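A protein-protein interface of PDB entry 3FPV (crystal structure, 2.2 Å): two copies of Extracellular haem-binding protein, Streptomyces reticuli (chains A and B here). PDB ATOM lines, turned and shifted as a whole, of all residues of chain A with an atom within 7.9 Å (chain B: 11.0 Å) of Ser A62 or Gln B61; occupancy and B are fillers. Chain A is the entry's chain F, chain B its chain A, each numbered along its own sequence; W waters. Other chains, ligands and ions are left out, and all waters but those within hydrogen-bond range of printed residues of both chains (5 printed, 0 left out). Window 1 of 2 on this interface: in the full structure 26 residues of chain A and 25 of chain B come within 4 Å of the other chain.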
ATOM      1  N   THR A  60      18.342  27.123  31.934  1.00  0.00           N
ATOM      2  CA  THR A  60      19.697  26.914  31.439  1.00  0.00           C
ATOM      3  C   THR A  60      19.856  27.481  30.027  1.00  0.00           C
ATOM      4  O   THR A  60      18.869  27.701  29.324  1.00  0.00           O
ATOM      5  CB  THR A  60      20.072  25.417  31.444  1.00  0.00           C
ATOM      6  OG1 THR A  60      21.399  25.248  30.929  1.00  0.00           O
ATOM      7  CG2 THR A  60      19.093  24.611  30.598  1.00  0.00           C
ATOM      8  N   GLN A  61      21.099  27.719  29.622  1.00  0.00           N
ATOM      9  CA  GLN A  61      21.380  28.295  28.311  1.00  0.00           C
ATOM     10  C   GLN A  61      22.006  27.265  27.376  1.00  0.00           C
ATOM     11  O   GLN A  61      22.758  26.394  27.811  1.00  0.00           O
ATOM     12  CB  GLN A  61      22.306  29.509  28.443  1.00  0.00           C
ATOM     13  CG  GLN A  61      21.712  30.669  29.229  1.00  0.00           C
ATOM     14  CD  GLN A  61      21.315  31.838  28.343  1.00  0.00           C
ATOM     15  OE1 GLN A  61      21.928  32.905  28.392  1.00  0.00           O
ATOM     16  NE2 GLN A  61      20.284  31.641  27.529  1.00  0.00           N
ATOM     17  N   SER A  62      21.690  27.373  26.089  1.00  0.00           N
ATOM     18  CA  SER A  62      22.401  26.621  25.061  1.00  0.00           C
ATOM     19  C   SER A  62      22.895  27.534  23.941  1.00  0.00           C
ATOM     20  O   SER A  62      22.324  28.596  23.696  1.00  0.00           O
ATOM     21  CB  SER A  62      21.506  25.519  24.489  1.00  0.00           C
ATOM     22  OG  SER A  62      20.487  26.062  23.665  1.00  0.00           O
ATOM     23  N   THR A  63      23.957  27.107  23.264  1.00  0.00           N
ATOM     24  CA  THR A  63      24.622  27.933  22.261  1.00  0.00           C
ATOM     25  C   THR A  63      24.421  27.365  20.856  1.00  0.00           C
ATOM     26  O   THR A  63      24.471  26.152  20.653  1.00  0.00           O
ATOM     27  CB  THR A  63      26.133  28.068  22.558  1.00  0.00           C
ATOM     28  OG1 THR A  63      26.317  28.550  23.895  1.00  0.00           O
ATOM     29  CG2 THR A  63      26.794  29.033  21.580  1.00  0.00           C
ATOM     30  N   HIS A  64      24.187  28.254  19.894  1.00  0.00           N
ATOM     31  CA  HIS A  64      23.897  27.854  18.520  1.00  0.00           C
ATOM     32  C   HIS A  64      24.705  28.690  17.540  1.00  0.00           C
ATOM     33  O   HIS A  64      25.087  29.819  17.846  1.00  0.00           O
ATOM     34  CB  HIS A  64      22.405  28.009  18.219  1.00  0.00           C
ATOM     35  CG  HIS A  64      21.514  27.480  19.298  1.00  0.00           C
ATOM     36  ND1 HIS A  64      21.078  26.173  19.329  1.00  0.00           N
ATOM     37  CD2 HIS A  64      20.979  28.082  20.387  1.00  0.00           C
ATOM     38  CE1 HIS A  64      20.312  25.992  20.390  1.00  0.00           C
ATOM     39  NE2 HIS A  64      20.236  27.135  21.049  1.00  0.00           N
ATOM     40  N   LEU A  65      24.960  28.133  16.361  1.00  0.00           N
ATOM     41  CA  LEU A  65      25.117  28.935  15.156  1.00  0.00           C
ATOM     42  C   LEU A  65      23.917  29.849  14.948  1.00  0.00           C
ATOM     43  O   LEU A  65      22.772  29.450  15.168  1.00  0.00           O
ATOM     44  CB  LEU A  65      25.311  28.040  13.932  1.00  0.00           C
ATOM     45  CG  LEU A  65      26.586  27.195  13.890  1.00  0.00           C
ATOM     46  CD1 LEU A  65      26.720  26.508  12.541  1.00  0.00           C
ATOM     47  CD2 LEU A  65      27.814  28.044  14.188  1.00  0.00           C
ATOM     48  N   THR A  66      24.186  31.081  14.526  1.00  0.00           N
ATOM     49  CA  THR A  66      23.183  31.901  13.856  1.00  0.00           C
ATOM     50  C   THR A  66      22.779  31.274  12.529  1.00  0.00           C
ATOM     51  O   THR A  66      23.552  30.527  11.927  1.00  0.00           O
ATOM     52  CB  THR A  66      23.697  33.330  13.604  1.00  0.00           C
ATOM     53  OG1 THR A  66      24.898  33.277  12.824  1.00  0.00           O
ATOM     54  CG2 THR A  66      23.984  34.035  14.921  1.00  0.00           C
ATOM     55  N   ASP A  94      21.291  21.661  13.824  1.00  0.00           N
ATOM     56  CA  ASP A  94      21.603  22.046  15.200  1.00  0.00           C
ATOM     57  C   ASP A  94      21.897  20.833  16.087  1.00  0.00           C
ATOM     58  O   ASP A  94      21.493  19.714  15.781  1.00  0.00           O
ATOM     59  CB  ASP A  94      20.452  22.863  15.792  1.00  0.00           C
ATOM     60  CG  ASP A  94      20.887  23.727  16.960  1.00  0.00           C
ATOM     61  OD1 ASP A  94      21.132  24.933  16.750  1.00  0.00           O
ATOM     62  OD2 ASP A  94      20.983  23.200  18.089  1.00  0.00           O
ATOM     63  N   ARG A  95      22.600  21.067  17.189  1.00  0.00           N
ATOM     64  CA  ARG A  95      22.785  20.050  18.222  1.00  0.00           C
ATOM     65  C   ARG A  95      21.461  19.568  18.823  1.00  0.00           C
ATOM     66  O   ARG A  95      21.401  18.501  19.433  1.00  0.00           O
ATOM     67  CB  ARG A  95      23.722  20.571  19.319  1.00  0.00           C
ATOM     68  CG  ARG A  95      23.719  19.760  20.609  1.00  0.00           C
ATOM     69  CD  ARG A  95      24.524  18.476  20.468  1.00  0.00           C
ATOM     70  NE  ARG A  95      24.615  17.747  21.731  1.00  0.00           N
ATOM     71  CZ  ARG A  95      25.198  16.561  21.869  1.00  0.00           C
ATOM     72  NH1 ARG A  95      25.745  15.959  20.819  1.00  0.00           N
ATOM     73  NH2 ARG A  95      25.234  15.973  23.059  1.00  0.00           N
ATOM     74  N   ASN A  96      20.398  20.349  18.642  1.00  0.00           N
ATOM     75  CA  ASN A  96      19.110  20.029  19.259  1.00  0.00           C
ATOM     76  C   ASN A  96      18.184  19.166  18.395  1.00  0.00           C
ATOM     77  O   ASN A  96      16.974  19.134  18.616  1.00  0.00           O
ATOM     78  CB  ASN A  96      18.388  21.305  19.716  1.00  0.00           C
ATOM     79  CG  ASN A  96      17.993  22.211  18.558  1.00  0.00           C
ATOM     80  OD1 ASN A  96      17.932  21.782  17.407  1.00  0.00           O
ATOM     81  ND2 ASN A  96      17.719  23.473  18.864  1.00  0.00           N
ATOM     82  N   LYS A 161      33.072  26.559  22.219  1.00  0.00           N
ATOM     83  CA  LYS A 161      33.608  26.337  23.560  1.00  0.00           C
ATOM     84  C   LYS A 161      33.609  24.854  23.930  1.00  0.00           C
ATOM     85  O   LYS A 161      33.213  24.479  25.035  1.00  0.00           O
ATOM     86  CB  LYS A 161      32.813  27.142  24.594  1.00  0.00           C
ATOM     87  CG  LYS A 161      32.567  28.594  24.199  1.00  0.00           C
ATOM     88  CD  LYS A 161      31.274  29.124  24.809  1.00  0.00           C
ATOM     89  CE  LYS A 161      30.851  30.435  24.157  1.00  0.00           C
ATOM     90  NZ  LYS A 161      31.968  31.425  24.105  1.00  0.00           N
ATOM     91  N   VAL A 165      27.709  22.208  18.531  1.00  0.00           N
ATOM     92  CA  VAL A 165      26.572  23.113  18.383  1.00  0.00           C
ATOM     93  C   VAL A 165      25.824  22.911  17.066  1.00  0.00           C
ATOM     94  O   VAL A 165      24.635  23.212  16.970  1.00  0.00           O
ATOM     95  CB  VAL A 165      26.987  24.596  18.529  1.00  0.00           C
ATOM     96  CG1 VAL A 165      27.382  24.895  19.966  1.00  0.00           C
ATOM     97  CG2 VAL A 165      28.123  24.938  17.573  1.00  0.00           C
ATOM     98  N   ALA B  54      33.404  27.556  16.199  1.00  0.00           N
ATOM     99  CA  ALA B  54      32.787  28.861  15.979  1.00  0.00           C
ATOM    100  C   ALA B  54      32.983  29.806  17.161  1.00  0.00           C
ATOM    101  O   ALA B  54      33.049  29.373  18.314  1.00  0.00           O
ATOM    102  CB  ALA B  54      31.305  28.698  15.668  1.00  0.00           C
ATOM    103  N   ARG B  55      33.070  31.100  16.864  1.00  0.00           N
ATOM    104  CA  ARG B  55      32.945  32.142  17.879  1.00  0.00           C
ATOM    105  C   ARG B  55      32.571  33.483  17.252  1.00  0.00           C
ATOM    106  O   ARG B  55      32.342  33.573  16.046  1.00  0.00           O
ATOM    107  CB  ARG B  55      34.249  32.280  18.667  1.00  0.00           C
ATOM    108  CG  ARG B  55      35.501  32.136  17.818  1.00  0.00           C
ATOM    109  CD  ARG B  55      36.659  32.898  18.427  1.00  0.00           C
ATOM    110  NE  ARG B  55      36.739  34.266  17.924  1.00  0.00           N
ATOM    111  CZ  ARG B  55      37.541  34.653  16.937  1.00  0.00           C
ATOM    112  NH1 ARG B  55      37.552  35.919  16.545  1.00  0.00           N
ATOM    113  NH2 ARG B  55      38.337  33.773  16.344  1.00  0.00           N
ATOM    114  N   GLY B  56      32.510  34.525  18.076  1.00  0.00           N
ATOM    115  CA  GLY B  56      31.365  34.747  18.950  1.00  0.00           C
ATOM    116  C   GLY B  56      30.212  35.421  18.231  1.00  0.00           C
ATOM    117  O   GLY B  56      29.057  35.298  18.639  1.00  0.00           O
ATOM    118  N   GLY B  57      30.530  36.136  17.155  1.00  0.00           N
ATOM    119  CA  GLY B  57      29.517  36.823  16.357  1.00  0.00           C
ATOM    120  C   GLY B  57      28.636  35.873  15.566  1.00  0.00           C
ATOM    121  O   GLY B  57      27.521  36.223  15.180  1.00  0.00           O
ATOM    122  N   GLU B  58      29.140  34.666  15.329  1.00  0.00           N
ATOM    123  CA  GLU B  58      28.373  33.636  14.639  1.00  0.00           C
ATOM    124  C   GLU B  58      27.669  32.713  15.627  1.00  0.00           C
ATOM    125  O   GLU B  58      26.973  31.778  15.230  1.00  0.00           O
ATOM    126  CB  GLU B  58      29.286  32.813  13.731  1.00  0.00           C
ATOM    127  CG  GLU B  58      30.457  33.584  13.153  1.00  0.00           C
ATOM    128  CD  GLU B  58      31.581  32.675  12.708  1.00  0.00           C
ATOM    129  OE1 GLU B  58      31.967  31.782  13.493  1.00  0.00           O
ATOM    130  OE2 GLU B  58      32.076  32.849  11.575  1.00  0.00           O
ATOM    131  N   LEU B  59      27.855  32.984  16.916  1.00  0.00           N
ATOM    132  CA  LEU B  59      27.083  32.329  17.965  1.00  0.00           C
ATOM    133  C   LEU B  59      25.849  33.130  18.364  1.00  0.00           C
ATOM    134  O   LEU B  59      25.867  34.362  18.362  1.00  0.00           O
ATOM    135  CB  LEU B  59      27.958  32.083  19.195  1.00  0.00           C
ATOM    136  CG  LEU B  59      29.253  31.302  18.969  1.00  0.00           C
ATOM    137  CD1 LEU B  59      29.990  31.103  20.284  1.00  0.00           C
ATOM    138  CD2 LEU B  59      28.966  29.968  18.300  1.00  0.00           C
ATOM    139  N   THR B  60      24.782  32.419  18.711  1.00  0.00           N
ATOM    140  CA  THR B  60      23.666  33.005  19.446  1.00  0.00           C
ATOM    141  C   THR B  60      23.187  32.064  20.552  1.00  0.00           C
ATOM    142  O   THR B  60      23.513  30.877  20.554  1.00  0.00           O
ATOM    143  CB  THR B  60      22.489  33.343  18.507  1.00  0.00           C
ATOM    144  OG1 THR B  60      21.394  33.860  19.272  1.00  0.00           O
ATOM    145  CG2 THR B  60      22.033  32.105  17.748  1.00  0.00           C
ATOM    146  N   GLN B  61      22.416  32.603  21.492  1.00  0.00           N
ATOM    147  CA  GLN B  61      22.032  31.866  22.692  1.00  0.00           C
ATOM    148  C   GLN B  61      20.518  31.689  22.770  1.00  0.00           C
ATOM    149  O   GLN B  61      19.762  32.512  22.256  1.00  0.00           O
ATOM    150  CB  GLN B  61      22.537  32.582  23.944  1.00  0.00           C
ATOM    151  CG  GLN B  61      24.035  32.464  24.171  1.00  0.00           C
ATOM    152  CD  GLN B  61      24.371  31.734  25.457  1.00  0.00           C
ATOM    153  OE1 GLN B  61      24.128  32.240  26.555  1.00  0.00           O
ATOM    154  NE2 GLN B  61      24.928  30.535  25.329  1.00  0.00           N
ATOM    155  N   SER B  62      20.082  30.612  23.416  1.00  0.00           N
ATOM    156  CA  SER B  62      18.677  30.458  23.784  1.00  0.00           C
ATOM    157  C   SER B  62      18.523  30.001  25.232  1.00  0.00           C
ATOM    158  O   SER B  62      19.452  29.446  25.819  1.00  0.00           O
ATOM    159  CB  SER B  62      17.977  29.477  22.840  1.00  0.00           C
ATOM    160  OG  SER B  62      18.683  28.251  22.761  1.00  0.00           O
ATOM    161  N   THR B  63      17.344  30.237  25.801  1.00  0.00           N
ATOM    162  CA  THR B  63      17.069  29.868  27.186  1.00  0.00           C
ATOM    163  C   THR B  63      16.025  28.755  27.266  1.00  0.00           C
ATOM    164  O   THR B  63      15.088  28.711  26.468  1.00  0.00           O
ATOM    165  CB  THR B  63      16.595  31.085  28.010  1.00  0.00           C
ATOM    166  OG1 THR B  63      17.597  32.107  27.972  1.00  0.00           O
ATOM    167  CG2 THR B  63      16.335  30.692  29.460  1.00  0.00           C
ATOM    168  N   HIS B  64      16.204  27.853  28.226  1.00  0.00           N
ATOM    169  CA  HIS B  64      15.356  26.673  28.356  1.00  0.00           C
ATOM    170  C   HIS B  64      15.120  26.345  29.826  1.00  0.00           C
ATOM    171  O   HIS B  64      15.939  26.678  30.681  1.00  0.00           O
ATOM    172  CB  HIS B  64      15.995  25.477  27.646  1.00  0.00           C
ATOM    173  CG  HIS B  64      16.414  25.764  26.238  1.00  0.00           C
ATOM    174  ND1 HIS B  64      15.548  25.667  25.170  1.00  0.00           N
ATOM    175  CD2 HIS B  64      17.604  26.155  25.723  1.00  0.00           C
ATOM    176  CE1 HIS B  64      16.187  25.983  24.058  1.00  0.00           C
ATOM    177  NE2 HIS B  64      17.436  26.283  24.366  1.00  0.00           N
ATOM    178  N   LEU B  65      13.997  25.693  30.114  1.00  0.00           N
ATOM    179  CA  LEU B  65      13.881  24.861  31.310  1.00  0.00           C
ATOM    180  C   LEU B  65      14.987  23.812  31.354  1.00  0.00           C
ATOM    181  O   LEU B  65      15.267  23.148  30.356  1.00  0.00           O
ATOM    182  CB  LEU B  65      12.510  24.181  31.367  1.00  0.00           C
ATOM    183  CG  LEU B  65      11.284  25.082  31.526  1.00  0.00           C
ATOM    184  CD1 LEU B  65      10.045  24.250  31.813  1.00  0.00           C
ATOM    185  CD2 LEU B  65      11.506  26.108  32.625  1.00  0.00           C
ATOM    186  N   THR B  66      15.614  23.670  32.516  1.00  0.00           N
ATOM    187  CA  THR B  66      16.275  22.423  32.888  1.00  0.00           C
ATOM    188  C   THR B  66      15.295  21.256  32.838  1.00  0.00           C
ATOM    189  O   THR B  66      14.092  21.440  33.026  1.00  0.00           O
ATOM    190  CB  THR B  66      16.875  22.506  34.301  1.00  0.00           C
ATOM    191  OG1 THR B  66      15.832  22.774  35.248  1.00  0.00           O
ATOM    192  CG2 THR B  66      17.916  23.614  34.377  1.00  0.00           C
ATOM    193  N   ASP B  94       9.861  21.768  24.709  1.00  0.00           N
ATOM    194  CA  ASP B  94      10.765  22.899  24.524  1.00  0.00           C
ATOM    195  C   ASP B  94      10.295  23.826  23.403  1.00  0.00           C
ATOM    196  O   ASP B  94       9.550  23.413  22.513  1.00  0.00           O
ATOM    197  CB  ASP B  94      12.182  22.396  24.235  1.00  0.00           C
ATOM    198  CG  ASP B  94      13.242  23.440  24.520  1.00  0.00           C
ATOM    199  OD1 ASP B  94      13.779  23.454  25.646  1.00  0.00           O
ATOM    200  OD2 ASP B  94      13.536  24.251  23.618  1.00  0.00           O
ATOM    201  N   ARG B  95      10.739  25.079  23.450  1.00  0.00           N
ATOM    202  CA  ARG B  95      10.480  26.038  22.378  1.00  0.00           C
ATOM    203  C   ARG B  95      11.106  25.620  21.043  1.00  0.00           C
ATOM    204  O   ARG B  95      10.767  26.164  19.992  1.00  0.00           O
ATOM    205  CB  ARG B  95      10.958  27.436  22.795  1.00  0.00           C
ATOM    206  CG  ARG B  95      11.108  28.435  21.656  1.00  0.00           C
ATOM    207  CD  ARG B  95       9.768  29.014  21.230  1.00  0.00           C
ATOM    208  NE  ARG B  95       9.935  30.072  20.238  1.00  0.00           N
ATOM    209  CZ  ARG B  95       8.932  30.704  19.637  1.00  0.00           C
ATOM    210  NH1 ARG B  95       7.675  30.388  19.921  1.00  0.00           N
ATOM    211  NH2 ARG B  95       9.185  31.654  18.748  1.00  0.00           N
ATOM    212  N   ASN B  96      12.007  24.641  21.083  1.00  0.00           N
ATOM    213  CA  ASN B  96      12.729  24.223  19.882  1.00  0.00           C
ATOM    214  C   ASN B  96      12.065  23.083  19.096  1.00  0.00           C
ATOM    215  O   ASN B  96      12.714  22.429  18.283  1.00  0.00           O
ATOM    216  CB  ASN B  96      14.193  23.886  20.209  1.00  0.00           C
ATOM    217  CG  ASN B  96      14.334  22.684  21.132  1.00  0.00           C
ATOM    218  OD1 ASN B  96      13.405  21.892  21.294  1.00  0.00           O
ATOM    219  ND2 ASN B  96      15.507  22.545  21.741  1.00  0.00           N
ATOM    220  N   ASN B  98      11.630  19.990  20.504  1.00  0.00           N
ATOM    221  CA  ASN B  98      11.722  18.711  21.197  1.00  0.00           C
ATOM    222  C   ASN B  98      10.828  18.605  22.428  1.00  0.00           C
ATOM    223  O   ASN B  98      10.735  19.538  23.226  1.00  0.00           O
ATOM    224  CB  ASN B  98      13.175  18.429  21.579  1.00  0.00           C
ATOM    225  CG  ASN B  98      14.139  18.738  20.455  1.00  0.00           C
ATOM    226  OD1 ASN B  98      13.841  18.494  19.283  1.00  0.00           O
ATOM    227  ND2 ASN B  98      15.299  19.283  20.802  1.00  0.00           N
ATOM    228  N   LEU B 100      10.542  17.350  26.076  1.00  0.00           N
ATOM    229  CA  LEU B 100      11.491  17.192  27.174  1.00  0.00           C
ATOM    230  C   LEU B 100      11.013  16.149  28.181  1.00  0.00           C
ATOM    231  O   LEU B 100      11.798  15.334  28.667  1.00  0.00           O
ATOM    232  CB  LEU B 100      11.703  18.528  27.890  1.00  0.00           C
ATOM    233  CG  LEU B 100      12.304  19.675  27.077  1.00  0.00           C
ATOM    234  CD1 LEU B 100      12.417  20.923  27.940  1.00  0.00           C
ATOM    235  CD2 LEU B 100      13.661  19.285  26.506  1.00  0.00           C
ATOM    236  N   ALA B 160      10.486  32.876  29.809  1.00  0.00           N
ATOM    237  CA  ALA B 160      11.584  33.466  30.567  1.00  0.00           C
ATOM    238  C   ALA B 160      11.895  34.877  30.079  1.00  0.00           C
ATOM    239  O   ALA B 160      12.227  35.080  28.908  1.00  0.00           O
ATOM    240  CB  ALA B 160      12.823  32.589  30.477  1.00  0.00           C
ATOM    241  N   LYS B 161      11.786  35.843  30.987  1.00  0.00           N
ATOM    242  CA  LYS B 161      11.801  37.262  30.633  1.00  0.00           C
ATOM    243  C   LYS B 161      10.996  37.542  29.365  1.00  0.00           C
ATOM    244  O   LYS B 161      11.477  38.203  28.444  1.00  0.00           O
ATOM    245  CB  LYS B 161      13.239  37.769  30.488  1.00  0.00           C
ATOM    246  CG  LYS B 161      13.852  38.258  31.793  1.00  0.00           C
ATOM    247  CD  LYS B 161      15.186  38.954  31.562  1.00  0.00           C
ATOM    248  CE  LYS B 161      16.311  37.946  31.350  1.00  0.00           C
ATOM    249  NZ  LYS B 161      17.517  38.578  30.744  1.00  0.00           N
ATOM    250  N   ALA B 163       9.797  35.770  26.904  1.00  0.00           N
ATOM    251  CA  ALA B 163       9.920  34.965  25.694  1.00  0.00           C
ATOM    252  C   ALA B 163       9.685  33.492  26.004  1.00  0.00           C
ATOM    253  O   ALA B 163      10.177  32.984  27.012  1.00  0.00           O
ATOM    254  CB  ALA B 163      11.292  35.164  25.069  1.00  0.00           C
ATOM    255  N   PRO B 164       8.930  32.796  25.135  1.00  0.00           N
ATOM    256  CA  PRO B 164       8.520  31.417  25.395  1.00  0.00           C
ATOM    257  C   PRO B 164       9.711  30.467  25.402  1.00  0.00           C
ATOM    258  O   PRO B 164      10.564  30.540  24.518  1.00  0.00           O
ATOM    259  CB  PRO B 164       7.597  31.097  24.215  1.00  0.00           C
ATOM    260  CG  PRO B 164       8.020  32.032  23.136  1.00  0.00           C
ATOM    261  CD  PRO B 164       8.425  33.289  23.841  1.00  0.00           C
ATOM    262  N   VAL B 165       9.769  29.589  26.400  1.00  0.00           N
ATOM    263  CA  VAL B 165      10.845  28.603  26.493  1.00  0.00           C
ATOM    264  C   VAL B 165      10.312  27.170  26.530  1.00  0.00           C
ATOM    265  O   VAL B 165      11.009  26.230  26.146  1.00  0.00           O
ATOM    266  CB  VAL B 165      11.751  28.850  27.724  1.00  0.00           C
ATOM    267  CG1 VAL B 165      12.373  30.237  27.656  1.00  0.00           C
ATOM    268  CG2 VAL B 165      10.968  28.675  29.018  1.00  0.00           C
HETATM  269  O   HOH W   1      17.168  26.829  20.159  1.00  0.00           O
HETATM  270  O   HOH W   2      18.826  33.657  25.655  1.00  0.00           O
HETATM  271  O   HOH W   3      17.777  24.407  21.644  1.00  0.00           O
HETATM  272  O   HOH W   4      26.358  35.686  12.686  1.00  0.00           O
HETATM  273  O   HOH W   5      19.369  31.528  30.711  1.00  0.00           O
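N of Thr A66 sits at hydrogen-bond distance from O of Glu B58 (3.0 Å).
The backbone carbonyl oxygen of His A64 is in hydrogen-bond range of the backbone NH of Thr B60, 2.8 Å away.
OE1 of Gln B61 lies close to OE1 of Gln A61, 2.9 Å away.
NE2 of Gln B61 lies within hydrogen-bond range of OG1 of Thr A63 (2.8 Å).
The side-chain amide nitrogen of Gln A61 is in hydrogen-bond range of the backbone carbonyl oxygen of Ser B62, at 2.9 Å.
The side-chain hydroxyl (OG) of Ser B62 is in hydrogen-bond range of the side-chain hydroxyl (OG) of Ser A62 (3.0 Å).
The side-chain hydroxyl (OG) of Ser B62 is in hydrogen-bond range of a ring nitrogen (NE2) of His A64 (2.6 Å).
The side-chain amide nitrogen of Gln A61 is in hydrogen-bond range of the side-chain hydroxyl of Thr B63 (2.8 Å).
The backbone carbonyl oxygen of His B64 lies within hydrogen-bond range of the backbone NH of Thr A60 (2.7 Å).
NE2 of His B64 sits at hydrogen-bond distance from OG of Ser A62 (3.1 Å).
ND2 of Asn B98 is in hydrogen-bond range of O of Asn A96, at 2.8 Å.
A ring nitrogen (NE2) of His B64 sits at hydrogen-bond distance from the side-chain hydroxyl (OG) of Ser B62 (2.8 Å).
A ring nitrogen (ND1) of His B64 is in hydrogen-bond range of the side-chain carboxylate of Asp B94 (2.9 Å).
The side-chain carboxylate of Asp B94 lies within hydrogen-bond range of the backbone NH of Asn B96, at 3.0 Å.
The side-chain amide oxygen (OD1) of Asn B96 is in hydrogen-bond range of the backbone NH (N) of Asn B98 (2.7 Å).
NE2 of His A64 is in hydrogen-bond range of OG of Ser A62, at 2.8 Å.
The side-chain carboxylate of Asp A94 sits at hydrogen-bond distance from a ring nitrogen (ND1) of His A64 (2.9 Å).
Thr A60 touches Ser B62.
Thr A60 touches Thr B63 (O to CA, 3.5 Å).
Ser A62 touches Gln B61 (O to CA, 3.4 Å).
Thr A63 touches Thr B60 (CA to O, 3.6 Å).
O of His A64 touches CA of Leu B59, 3.2 Å away.
Ala B54 touches Leu A65.
Leu A65 touches Thr B60 (O to CG2, 3.8 Å).
Thr A66 touches Leu B59.
CG2 of Thr B60 touches CG2 of Thr A66, at 3.9 Å.
Asn B96 touches Asn A96.
Ser A62 touches just these residues of chain B: Gln B61, Ser B62 and His B64.
Gln B61 touches three residues of chain A.
Of chain B, only Thr B60 and Gln B61 come within 4 Å of Thr A63.
Thr B60 touches four residues of chain A.
Of the printed residues of chain A, Ser B62 touches Thr A60, Gln A61, Ser A62 and His A64.
Of the printed residues of chain A, Ala B54 touches Leu A65.
Of the printed residues of chain A, Asn B98 touches Asn A96 (2.8 Å).
Of the printed residues of chain A, Leu B59 touches His A64 (3.2 Å) and Thr A66 (3.9 Å).
Arg B55 touches none of the printed residues of chain A.
The nearest residue of chain B that does not touch Ser A62 is Thr B60 (4.1 Å).
The nearest printed residue of chain B that does not touch Asn A96 is His B64 (6.0 Å).
Hydrophobic or aromatic side chains of chain B within 4 Å of the printed part of chain A: Ala B54, Leu B59 and His B64.
Printed residues of chain A that touch a printed residue of chain B: Thr A60, Gln A61, Ser A62, Thr A63, His A64, Leu A65, Thr A66 and Asn A96.
Hydrophobic or aromatic side chains of chain A within 4 Å of the printed part of chain B: His A64 and Leu A65.
Along chain A the printed residues that touch a printed residue of chain B span positions 60 to 96.
Among the printed residues, 23 pairs touch across the chains.
Thr A60 touches Thr B63, and with the chains exchanged Thr A63 touches Thr B60.
Gln A61 touches Thr B63, and with the chains exchanged Thr A63 touches Gln B61.
Ser A62 touches His B64, and with the chains exchanged His A64 touches Ser B62.
Thr A66 touches Thr B60, but with the chains exchanged Thr A60 does not touch Thr B66 (4.1 Å).
12 positions are printed for both chains.
Of the 23 pairs that touch across the chains among the printed residues, 13 have their exchanged pair printed and touching as well.
Water W4 lies within hydrogen-bond range of O of Gly B57 (2.8 Å) and OG1 of Thr A66 (2.8 Å).
Water W3 lies within hydrogen-bond range of the side-chain amide nitrogen (ND2) of Asn A96 (2.9 Å), the side-chain amide nitrogen (ND2) of Asn B96 (2.9 Å) and a ring nitrogen (NE2) of His B64 (3.3 Å).
Water W2 bridges OG1 of Thr B63 and NE2 of Gln A61.
Water W1 bridges NE2 of His A64 (3.2 Å) and OG of Ser B62 (3.3 Å).
Water W5 lies within hydrogen-bond range of the side-chain amide nitrogen of Gln A61 and the side-chain hydroxyl of Thr B63.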
